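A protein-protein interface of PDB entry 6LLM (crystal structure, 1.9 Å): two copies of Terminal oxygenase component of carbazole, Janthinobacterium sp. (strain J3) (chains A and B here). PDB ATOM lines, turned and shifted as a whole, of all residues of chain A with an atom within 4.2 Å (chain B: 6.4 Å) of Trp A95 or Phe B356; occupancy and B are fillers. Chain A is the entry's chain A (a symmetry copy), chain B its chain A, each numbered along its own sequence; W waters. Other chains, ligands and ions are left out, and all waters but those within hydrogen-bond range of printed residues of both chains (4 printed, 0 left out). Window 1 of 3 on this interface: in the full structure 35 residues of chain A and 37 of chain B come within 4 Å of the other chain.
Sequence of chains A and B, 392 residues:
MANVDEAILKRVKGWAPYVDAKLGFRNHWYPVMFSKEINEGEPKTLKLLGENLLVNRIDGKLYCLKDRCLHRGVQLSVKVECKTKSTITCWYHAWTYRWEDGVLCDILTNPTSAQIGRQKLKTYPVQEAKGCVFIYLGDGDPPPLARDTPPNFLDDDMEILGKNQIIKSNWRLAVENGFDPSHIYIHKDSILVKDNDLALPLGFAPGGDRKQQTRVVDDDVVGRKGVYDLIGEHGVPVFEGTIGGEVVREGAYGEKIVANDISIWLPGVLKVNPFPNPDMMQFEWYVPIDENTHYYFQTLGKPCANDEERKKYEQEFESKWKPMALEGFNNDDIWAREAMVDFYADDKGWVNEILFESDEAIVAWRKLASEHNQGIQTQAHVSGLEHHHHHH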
ATOM      1  N   LEU A  70      -2.578 -11.783   1.775  1.00  0.00           N
ATOM      2  CA  LEU A  70      -2.294 -10.463   2.312  1.00  0.00           C
ATOM      3  C   LEU A  70      -3.097  -9.374   1.615  1.00  0.00           C
ATOM      4  O   LEU A  70      -3.243  -8.301   2.142  1.00  0.00           O
ATOM      5  CB  LEU A  70      -0.791 -10.192   2.149  1.00  0.00           C
ATOM      6  CG  LEU A  70       0.152 -11.088   2.949  1.00  0.00           C
ATOM      7  CD1 LEU A  70       1.610 -10.735   2.656  1.00  0.00           C
ATOM      8  CD2 LEU A  70      -0.128 -10.982   4.437  1.00  0.00           C
ATOM      9  N   HIS A  71      -3.541  -9.623   0.376  1.00  0.00           N
ATOM     10  CA  HIS A  71      -4.187  -8.649  -0.439  1.00  0.00           C
ATOM     11  C   HIS A  71      -5.632  -8.344   0.078  1.00  0.00           C
ATOM     12  O   HIS A  71      -5.860  -7.280   0.673  1.00  0.00           O
ATOM     13  CB  HIS A  71      -4.158  -9.166  -1.872  1.00  0.00           C
ATOM     14  CG  HIS A  71      -4.738  -8.259  -2.886  1.00  0.00           C
ATOM     15  ND1 HIS A  71      -5.441  -8.722  -3.977  1.00  0.00           N
ATOM     16  CD2 HIS A  71      -4.782  -6.910  -2.934  1.00  0.00           C
ATOM     17  CE1 HIS A  71      -5.844  -7.675  -4.679  1.00  0.00           C
ATOM     18  NE2 HIS A  71      -5.430  -6.582  -4.084  1.00  0.00           N
ATOM     19  N   ILE A  88       2.870 -21.169  -3.855  1.00  0.00           N
ATOM     20  CA  ILE A  88       1.423 -21.211  -4.038  1.00  0.00           C
ATOM     21  C   ILE A  88       1.003 -19.847  -4.542  1.00  0.00           C
ATOM     22  O   ILE A  88       1.475 -18.824  -4.080  1.00  0.00           O
ATOM     23  CB  ILE A  88       0.667 -21.593  -2.721  1.00  0.00           C
ATOM     24  CG1 ILE A  88      -0.860 -21.609  -2.917  1.00  0.00           C
ATOM     25  CG2 ILE A  88       1.065 -20.688  -1.556  1.00  0.00           C
ATOM     26  CD1 ILE A  88      -1.612 -22.340  -1.733  1.00  0.00           C
ATOM     27  N   THR A  89       0.025 -19.853  -5.451  1.00  0.00           N
ATOM     28  CA  THR A  89      -0.499 -18.667  -6.076  1.00  0.00           C
ATOM     29  C   THR A  89      -1.969 -18.442  -5.635  1.00  0.00           C
ATOM     30  O   THR A  89      -2.823 -19.304  -5.838  1.00  0.00           O
ATOM     31  CB  THR A  89      -0.423 -18.841  -7.597  1.00  0.00           C
ATOM     32  OG1 THR A  89       0.949 -18.825  -8.025  1.00  0.00           O
ATOM     33  CG2 THR A  89      -1.142 -17.758  -8.330  1.00  0.00           C
ATOM     34  N   CYS A  90      -2.265 -17.285  -5.063  1.00  0.00           N
ATOM     35  CA  CYS A  90      -3.646 -16.989  -4.747  1.00  0.00           C
ATOM     36  C   CYS A  90      -4.483 -17.019  -6.029  1.00  0.00           C
ATOM     37  O   CYS A  90      -4.097 -16.458  -7.054  1.00  0.00           O
ATOM     38  CB  CYS A  90      -3.770 -15.611  -4.112  1.00  0.00           C
ATOM     39  SG  CYS A  90      -5.454 -15.178  -3.583  1.00  0.00           S
ATOM     40  N   HIS A  93      -6.010 -12.746  -7.423  1.00  0.00           N
ATOM     41  CA  HIS A  93      -5.163 -11.838  -8.258  1.00  0.00           C
ATOM     42  C   HIS A  93      -3.721 -12.353  -8.391  1.00  0.00           C
ATOM     43  O   HIS A  93      -2.795 -11.631  -8.770  1.00  0.00           O
ATOM     44  CB  HIS A  93      -5.179 -10.436  -7.668  1.00  0.00           C
ATOM     45  CG  HIS A  93      -6.517  -9.961  -7.204  1.00  0.00           C
ATOM     46  ND1 HIS A  93      -7.010 -10.250  -5.921  1.00  0.00           N
ATOM     47  CD2 HIS A  93      -7.448  -9.201  -7.820  1.00  0.00           C
ATOM     48  CE1 HIS A  93      -8.199  -9.671  -5.810  1.00  0.00           C
ATOM     49  NE2 HIS A  93      -8.494  -9.023  -6.952  1.00  0.00           N
ATOM     50  N   ALA A  94      -3.526 -13.612  -8.064  1.00  0.00           N
ATOM     51  CA  ALA A  94      -2.308 -14.369  -8.329  1.00  0.00           C
ATOM     52  C   ALA A  94      -1.089 -13.817  -7.571  1.00  0.00           C
ATOM     53  O   ALA A  94       0.024 -14.013  -8.043  1.00  0.00           O
ATOM     54  CB  ALA A  94      -2.032 -14.439  -9.825  1.00  0.00           C
ATOM     55  N   TRP A  95      -1.283 -13.215  -6.393  1.00  0.00           N
ATOM     56  CA  TRP A  95      -0.148 -13.055  -5.469  1.00  0.00           C
ATOM     57  C   TRP A  95       0.445 -14.439  -5.160  1.00  0.00           C
ATOM     58  O   TRP A  95      -0.258 -15.370  -4.824  1.00  0.00           O
ATOM     59  CB  TRP A  95      -0.563 -12.294  -4.188  1.00  0.00           C
ATOM     60  CG  TRP A  95      -0.891 -10.852  -4.389  1.00  0.00           C
ATOM     61  CD1 TRP A  95      -1.446 -10.248  -5.477  1.00  0.00           C
ATOM     62  CD2 TRP A  95      -0.742  -9.825  -3.412  1.00  0.00           C
ATOM     63  NE1 TRP A  95      -1.655  -8.921  -5.226  1.00  0.00           N
ATOM     64  CE2 TRP A  95      -1.209  -8.627  -3.985  1.00  0.00           C
ATOM     65  CE3 TRP A  95      -0.223  -9.787  -2.118  1.00  0.00           C
ATOM     66  CZ2 TRP A  95      -1.209  -7.421  -3.297  1.00  0.00           C
ATOM     67  CZ3 TRP A  95      -0.269  -8.594  -1.425  1.00  0.00           C
ATOM     68  CH2 TRP A  95      -0.746  -7.447  -2.001  1.00  0.00           C
ATOM     69  N   THR A  96       1.779 -14.595  -5.295  1.00  0.00           N
ATOM     70  CA  THR A  96       2.440 -15.865  -5.225  1.00  0.00           C
ATOM     71  C   THR A  96       3.458 -15.826  -4.093  1.00  0.00           C
ATOM     72  O   THR A  96       4.325 -14.905  -4.027  1.00  0.00           O
ATOM     73  CB  THR A  96       3.105 -16.203  -6.577  1.00  0.00           C
ATOM     74  OG1 THR A  96       2.052 -16.292  -7.549  1.00  0.00           O
ATOM     75  CG2 THR A  96       3.858 -17.514  -6.548  1.00  0.00           C
ATOM     76  N   TYR A  97       3.371 -16.830  -3.225  1.00  0.00           N
ATOM     77  CA  TYR A  97       4.120 -16.930  -1.994  1.00  0.00           C
ATOM     78  C   TYR A  97       5.007 -18.186  -2.009  1.00  0.00           C
ATOM     79  O   TYR A  97       4.631 -19.209  -2.493  1.00  0.00           O
ATOM     80  CB  TYR A  97       3.203 -16.962  -0.766  1.00  0.00           C
ATOM     81  CG  TYR A  97       2.203 -15.846  -0.681  1.00  0.00           C
ATOM     82  CD1 TYR A  97       0.940 -15.971  -1.251  1.00  0.00           C
ATOM     83  CD2 TYR A  97       2.506 -14.656  -0.053  1.00  0.00           C
ATOM     84  CE1 TYR A  97       0.009 -14.954  -1.170  1.00  0.00           C
ATOM     85  CE2 TYR A  97       1.564 -13.657   0.089  1.00  0.00           C
ATOM     86  CZ  TYR A  97       0.309 -13.787  -0.492  1.00  0.00           C
ATOM     87  OH  TYR A  97      -0.596 -12.781  -0.385  1.00  0.00           O
ATOM     88  N   LEU A 104       6.283 -12.987  -0.600  1.00  0.00           N
ATOM     89  CA  LEU A 104       5.611 -12.682  -1.824  1.00  0.00           C
ATOM     90  C   LEU A 104       6.676 -12.534  -2.926  1.00  0.00           C
ATOM     91  O   LEU A 104       7.311 -11.465  -3.004  1.00  0.00           O
ATOM     92  CB  LEU A 104       4.816 -11.400  -1.636  1.00  0.00           C
ATOM     93  CG  LEU A 104       4.059 -10.880  -2.853  1.00  0.00           C
ATOM     94  CD1 LEU A 104       2.950 -11.821  -3.338  1.00  0.00           C
ATOM     95  CD2 LEU A 104       3.491  -9.482  -2.566  1.00  0.00           C
ATOM     96  N   ASP A 106       6.192 -13.231  -6.442  1.00  0.00           N
ATOM     97  CA  ASP A 106       5.711 -12.871  -7.779  1.00  0.00           C
ATOM     98  C   ASP A 106       4.217 -12.499  -7.690  1.00  0.00           C
ATOM     99  O   ASP A 106       3.561 -12.879  -6.674  1.00  0.00           O
ATOM    100  CB  ASP A 106       5.868 -14.041  -8.734  1.00  0.00           C
ATOM    101  CG  ASP A 106       7.293 -14.191  -9.300  1.00  0.00           C
ATOM    102  OD1 ASP A 106       7.781 -13.234 -10.021  1.00  0.00           O
ATOM    103  OD2 ASP A 106       7.946 -15.213  -8.892  1.00  0.00           O
ATOM    104  N   ILE A 107       3.745 -11.701  -8.626  1.00  0.00           N
ATOM    105  CA  ILE A 107       2.305 -11.428  -8.807  1.00  0.00           C
ATOM    106  C   ILE A 107       2.027 -11.600 -10.282  1.00  0.00           C
ATOM    107  O   ILE A 107       2.416 -10.754 -11.085  1.00  0.00           O
ATOM    108  CB  ILE A 107       1.828 -10.069  -8.287  1.00  0.00           C
ATOM    109  CG1 ILE A 107       2.146  -9.879  -6.805  1.00  0.00           C
ATOM    110  CG2 ILE A 107       0.335  -9.942  -8.547  1.00  0.00           C
ATOM    111  CD1 ILE A 107       1.898  -8.489  -6.296  1.00  0.00           C
ATOM    112  N   THR A 109      -0.584 -11.224 -12.030  1.00  0.00           N
ATOM    113  CA  THR A 109      -1.416 -10.210 -12.620  1.00  0.00           C
ATOM    114  C   THR A 109      -0.675  -8.897 -12.813  1.00  0.00           C
ATOM    115  O   THR A 109      -1.219  -8.010 -13.440  1.00  0.00           O
ATOM    116  CB  THR A 109      -2.705  -9.929 -11.821  1.00  0.00           C
ATOM    117  OG1 THR A 109      -2.326  -9.610 -10.482  1.00  0.00           O
ATOM    118  CG2 THR A 109      -3.623 -11.129 -11.887  1.00  0.00           C
ATOM    119  N   ASN A 110       0.518  -8.732 -12.223  1.00  0.00           N
ATOM    120  CA  ASN A 110       1.256  -7.494 -12.379  1.00  0.00           C
ATOM    121  C   ASN A 110       2.678  -7.730 -11.930  1.00  0.00           C
ATOM    122  O   ASN A 110       3.026  -7.425 -10.791  1.00  0.00           O
ATOM    123  CB  ASN A 110       0.673  -6.305 -11.602  1.00  0.00           C
ATOM    124  CG  ASN A 110       1.515  -5.070 -11.776  1.00  0.00           C
ATOM    125  OD1 ASN A 110       2.441  -5.035 -12.623  1.00  0.00           O
ATOM    126  ND2 ASN A 110       1.223  -4.056 -10.995  1.00  0.00           N
ATOM    127  N   SER A 113       4.640  -5.019 -10.010  1.00  0.00           N
ATOM    128  CA  SER A 113       4.156  -4.472  -8.792  1.00  0.00           C
ATOM    129  C   SER A 113       5.322  -4.196  -7.821  1.00  0.00           C
ATOM    130  O   SER A 113       6.210  -5.055  -7.573  1.00  0.00           O
ATOM    131  CB  SER A 113       3.135  -5.368  -8.134  1.00  0.00           C
ATOM    132  OG  SER A 113       2.780  -4.798  -6.882  1.00  0.00           O
ATOM    133  N   GLN A 115       4.960  -4.315  -4.703  1.00  0.00           N
ATOM    134  CA  GLN A 115       4.745  -5.176  -3.572  1.00  0.00           C
ATOM    135  C   GLN A 115       5.649  -6.398  -3.625  1.00  0.00           C
ATOM    136  O   GLN A 115       5.956  -6.950  -2.575  1.00  0.00           O
ATOM    137  CB  GLN A 115       3.267  -5.614  -3.445  1.00  0.00           C
ATOM    138  CG  GLN A 115       2.304  -4.466  -3.129  1.00  0.00           C
ATOM    139  CD  GLN A 115       2.460  -3.859  -1.749  1.00  0.00           C
ATOM    140  OE1 GLN A 115       3.469  -4.032  -1.045  1.00  0.00           O
ATOM    141  NE2 GLN A 115       1.446  -3.108  -1.337  1.00  0.00           N
ATOM    142  N   ASP B 180     -12.636  -4.519 -10.443  1.00  0.00           N
ATOM    143  CA  ASP B 180     -11.283  -4.808 -10.045  1.00  0.00           C
ATOM    144  C   ASP B 180     -10.464  -5.269 -11.258  1.00  0.00           C
ATOM    145  O   ASP B 180     -10.711  -6.334 -11.803  1.00  0.00           O
ATOM    146  CB  ASP B 180     -11.400  -5.855  -8.949  1.00  0.00           C
ATOM    147  CG  ASP B 180     -10.100  -6.394  -8.424  1.00  0.00           C
ATOM    148  OD1 ASP B 180      -9.111  -6.286  -9.172  1.00  0.00           O
ATOM    149  OD2 ASP B 180     -10.167  -7.047  -7.316  1.00  0.00           O
ATOM    150  N   SER B 182      -7.513  -6.518 -11.891  1.00  0.00           N
ATOM    151  CA  SER B 182      -6.700  -7.683 -11.832  1.00  0.00           C
ATOM    152  C   SER B 182      -7.551  -8.937 -11.575  1.00  0.00           C
ATOM    153  O   SER B 182      -7.053 -10.044 -11.706  1.00  0.00           O
ATOM    154  CB  SER B 182      -5.631  -7.542 -10.818  1.00  0.00           C
ATOM    155  OG  SER B 182      -4.648  -6.608 -11.245  1.00  0.00           O
ATOM    156  N   ILE B 354      -4.100  -5.180   2.108  1.00  0.00           N
ATOM    157  CA  ILE B 354      -2.913  -4.532   1.494  1.00  0.00           C
ATOM    158  C   ILE B 354      -3.153  -4.429  -0.002  1.00  0.00           C
ATOM    159  O   ILE B 354      -3.063  -5.415  -0.695  1.00  0.00           O
ATOM    160  CB  ILE B 354      -1.623  -5.307   1.817  1.00  0.00           C
ATOM    161  CG1 ILE B 354      -1.399  -5.430   3.315  1.00  0.00           C
ATOM    162  CG2 ILE B 354      -0.403  -4.687   1.101  1.00  0.00           C
ATOM    163  CD1 ILE B 354      -0.306  -6.440   3.706  1.00  0.00           C
ATOM    164  N   LEU B 355      -3.410  -3.230  -0.471  1.00  0.00           N
ATOM    165  CA  LEU B 355      -3.770  -2.982  -1.873  1.00  0.00           C
ATOM    166  C   LEU B 355      -2.505  -2.888  -2.738  1.00  0.00           C
ATOM    167  O   LEU B 355      -1.430  -2.733  -2.216  1.00  0.00           O
ATOM    168  CB  LEU B 355      -4.567  -1.680  -1.950  1.00  0.00           C
ATOM    169  CG  LEU B 355      -5.892  -1.696  -1.194  1.00  0.00           C
ATOM    170  CD1 LEU B 355      -6.654  -0.430  -1.478  1.00  0.00           C
ATOM    171  CD2 LEU B 355      -6.690  -2.944  -1.555  1.00  0.00           C
ATOM    172  N   PHE B 356      -2.660  -3.159  -4.031  1.00  0.00           N
ATOM    173  CA  PHE B 356      -1.581  -2.975  -5.029  1.00  0.00           C
ATOM    174  C   PHE B 356      -2.097  -2.060  -6.144  1.00  0.00           C
ATOM    175  O   PHE B 356      -3.178  -1.473  -6.016  1.00  0.00           O
ATOM    176  CB  PHE B 356      -0.898  -4.294  -5.406  1.00  0.00           C
ATOM    177  CG  PHE B 356      -1.604  -5.205  -6.382  1.00  0.00           C
ATOM    178  CD1 PHE B 356      -2.968  -5.421  -6.363  1.00  0.00           C
ATOM    179  CD2 PHE B 356      -0.872  -5.901  -7.311  1.00  0.00           C
ATOM    180  CE1 PHE B 356      -3.572  -6.285  -7.267  1.00  0.00           C
ATOM    181  CE2 PHE B 356      -1.478  -6.770  -8.213  1.00  0.00           C
ATOM    182  CZ  PHE B 356      -2.821  -6.967  -8.193  1.00  0.00           C
ATOM    183  N   GLU B 357      -1.292  -1.912  -7.188  1.00  0.00           N
ATOM    184  CA  GLU B 357      -1.430  -0.777  -8.118  1.00  0.00           C
ATOM    185  C   GLU B 357      -2.798  -0.791  -8.806  1.00  0.00           C
ATOM    186  O   GLU B 357      -3.388   0.249  -8.934  1.00  0.00           O
ATOM    187  CB  GLU B 357      -0.267  -0.785  -9.134  1.00  0.00           C
ATOM    188  CG  GLU B 357       1.067  -0.412  -8.490  1.00  0.00           C
ATOM    189  CD  GLU B 357       1.903  -1.525  -7.854  1.00  0.00           C
ATOM    190  OE1 GLU B 357       1.382  -2.660  -7.623  1.00  0.00           O
ATOM    191  OE2 GLU B 357       3.120  -1.268  -7.604  1.00  0.00           O
ATOM    192  N   SER B 358      -3.270  -1.955  -9.276  1.00  0.00           N
ATOM    193  CA  SER B 358      -4.494  -1.969 -10.047  1.00  0.00           C
ATOM    194  C   SER B 358      -5.685  -1.626  -9.158  1.00  0.00           C
ATOM    195  O   SER B 358      -6.685  -1.307  -9.665  1.00  0.00           O
ATOM    196  CB  SER B 358      -4.718  -3.258 -10.741  1.00  0.00           C
ATOM    197  OG  SER B 358      -4.746  -4.362  -9.825  1.00  0.00           O
ATOM    198  N   ASP B 359      -5.528  -1.668  -7.831  1.00  0.00           N
ATOM    199  CA  ASP B 359      -6.603  -1.268  -6.941  1.00  0.00           C
ATOM    200  C   ASP B 359      -6.831   0.245  -6.953  1.00  0.00           C
ATOM    201  O   ASP B 359      -7.706   0.724  -6.296  1.00  0.00           O
ATOM    202  CB  ASP B 359      -6.296  -1.768  -5.535  1.00  0.00           C
ATOM    203  CG  ASP B 359      -6.270  -3.284  -5.426  1.00  0.00           C
ATOM    204  OD1 ASP B 359      -7.105  -3.919  -6.090  1.00  0.00           O
ATOM    205  OD2 ASP B 359      -5.422  -3.806  -4.672  1.00  0.00           O
ATOM    206  N   GLU B 360      -6.024   1.018  -7.686  1.00  0.00           N
ATOM    207  CA  GLU B 360      -6.311   2.473  -7.805  1.00  0.00           C
ATOM    208  C   GLU B 360      -7.751   2.683  -8.305  1.00  0.00           C
ATOM    209  O   GLU B 360      -8.439   3.621  -7.882  1.00  0.00           O
ATOM    210  CB  GLU B 360      -5.296   3.125  -8.753  1.00  0.00           C
ATOM    211  CG  GLU B 360      -5.543   4.595  -8.995  1.00  0.00           C
ATOM    212  CD  GLU B 360      -5.753   5.464  -7.752  1.00  0.00           C
ATOM    213  OE1 GLU B 360      -5.079   5.180  -6.698  1.00  0.00           O
ATOM    214  OE2 GLU B 360      -6.674   6.379  -7.806  1.00  0.00           O
HETATM  215  O   HOH W   1      -2.578  -5.147 -12.376  1.00  0.00           O
HETATM  216  O   HOH W   2      -8.691  -6.052  -5.205  1.00  0.00           O
HETATM  217  O   HOH W   3       3.044  -1.686 -11.030  1.00  0.00           O
HETATM  218  O   HOH W   4      -1.506  -4.158 -10.028  1.00  0.00           O
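Of the 9 printed residues of chain B, 7 touch a printed residue of chain A. Printed residues of chain B that touch a printed residue of chain A: Asp B180, Ser B182, Ile B354, Leu B355, Phe B356, Glu B357 and Asp B359. Hydrophobic or aromatic side chains of chain B within 4 Å of the printed part of chain A: Ile B354 and Phe B356. Among the printed residues, no Asp or Glu carboxylate lies within 4 Å of a Lys or Arg side-chain nitrogen of the other chain.
OE1 of Glu B357 sits at hydrogen-bond distance from OG of Ser A113. The side-chain amide nitrogen (NE2) of Gln A115 is in hydrogen-bond range of the backbone carbonyl oxygen (O) of Leu B355 (3.0 Å). N of Ile B354 lies within hydrogen-bond range of O of Leu A70, at 3.2 Å. The backbone NH (N) of Ile B354 lies within hydrogen-bond range of the backbone carbonyl oxygen (O) of His A71. OD2 of Asp B180 sits at hydrogen-bond distance from NE2 of His A93, 2.6 Å away. A ring nitrogen (NE2) of His A71 sits at hydrogen-bond distance from the side-chain carboxylate (OD2) of Asp B359 (2.8 Å).
The side-chain amide oxygen (OD1) of Asn A110 sits at hydrogen-bond distance from the backbone NH (N) of Ser A113, at 3.4 Å. The side-chain carboxylate (OD2) of Asp B359 is in hydrogen-bond range of the backbone NH (N) of Phe B356. The side-chain hydroxyl (OG) of Ser B182 is in hydrogen-bond range of the side-chain hydroxyl (OG) of Ser B358, 2.7 Å away. The backbone NH (N) of Leu A70 sits at hydrogen-bond distance from the side-chain hydroxyl (OH) of Tyr A97 (3.1 Å). N of Ser B182 lies within hydrogen-bond range of OD1 of Asp B180 (3.2 Å). OG of Ser A113 sits at hydrogen-bond distance from N of Gln A115 (3.1 Å).
Water W2 lies within hydrogen-bond range of OD2 of Asp B180, OD1 of Asp B359, NE2 of His A93 and NE2 of His A71. Water W1 lies within hydrogen-bond range of the side-chain hydroxyl of Ser B182 (2.8 Å), the backbone carbonyl oxygen of Thr A109 (3.3 Å) and the side-chain hydroxyl of Ser B358 (3.4 Å). Water W4 lies within hydrogen-bond range of ND2 of Asn A110 (2.9 Å) and N of Ser B358 (2.9 Å). Water W3 lies within hydrogen-bond range of the side-chain amide nitrogen of Asn A110 (3.0 Å) and the side-chain carboxylate of Glu B357 (3.5 Å).
Among the printed residues, merely in contact across the chains: Trp A95 with Ile B354, Gln A115 with Ile B354, Thr A109 with Phe B356, His A71 with Phe B356, Thr A109 with Ser B182, Asn A110 with Glu B357, Ile A107 with Phe B356, Trp A95 with Phe B356, His A93 with Ser B182, Ser A113 with Phe B356 and Gln A115 with Phe B356.
No position is printed for both chains. Of the 17 pairs that touch across the chains among the printed residues, none has its exchanged pair printed and touching as well.
Trp A95 touches just these residues of chain B: Ile B354 and Phe B356. Printed residues of chain A within 4 Å of Asp B359: His A71 (2.8 Å). Printed residues of chain A within 4 Å of Ser B182: His A93 and Thr A109. Of the printed residues of chain B, Ile A107 touches Phe B356. Of the printed residues of chain B, Ser A113 touches Phe B356 and Glu B357. Of the printed residues of chain B, Thr A109 touches Ser B182 and Phe B356. The nearest residue of chain B that does not touch Trp A95 is Leu B355 (4.7 Å).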
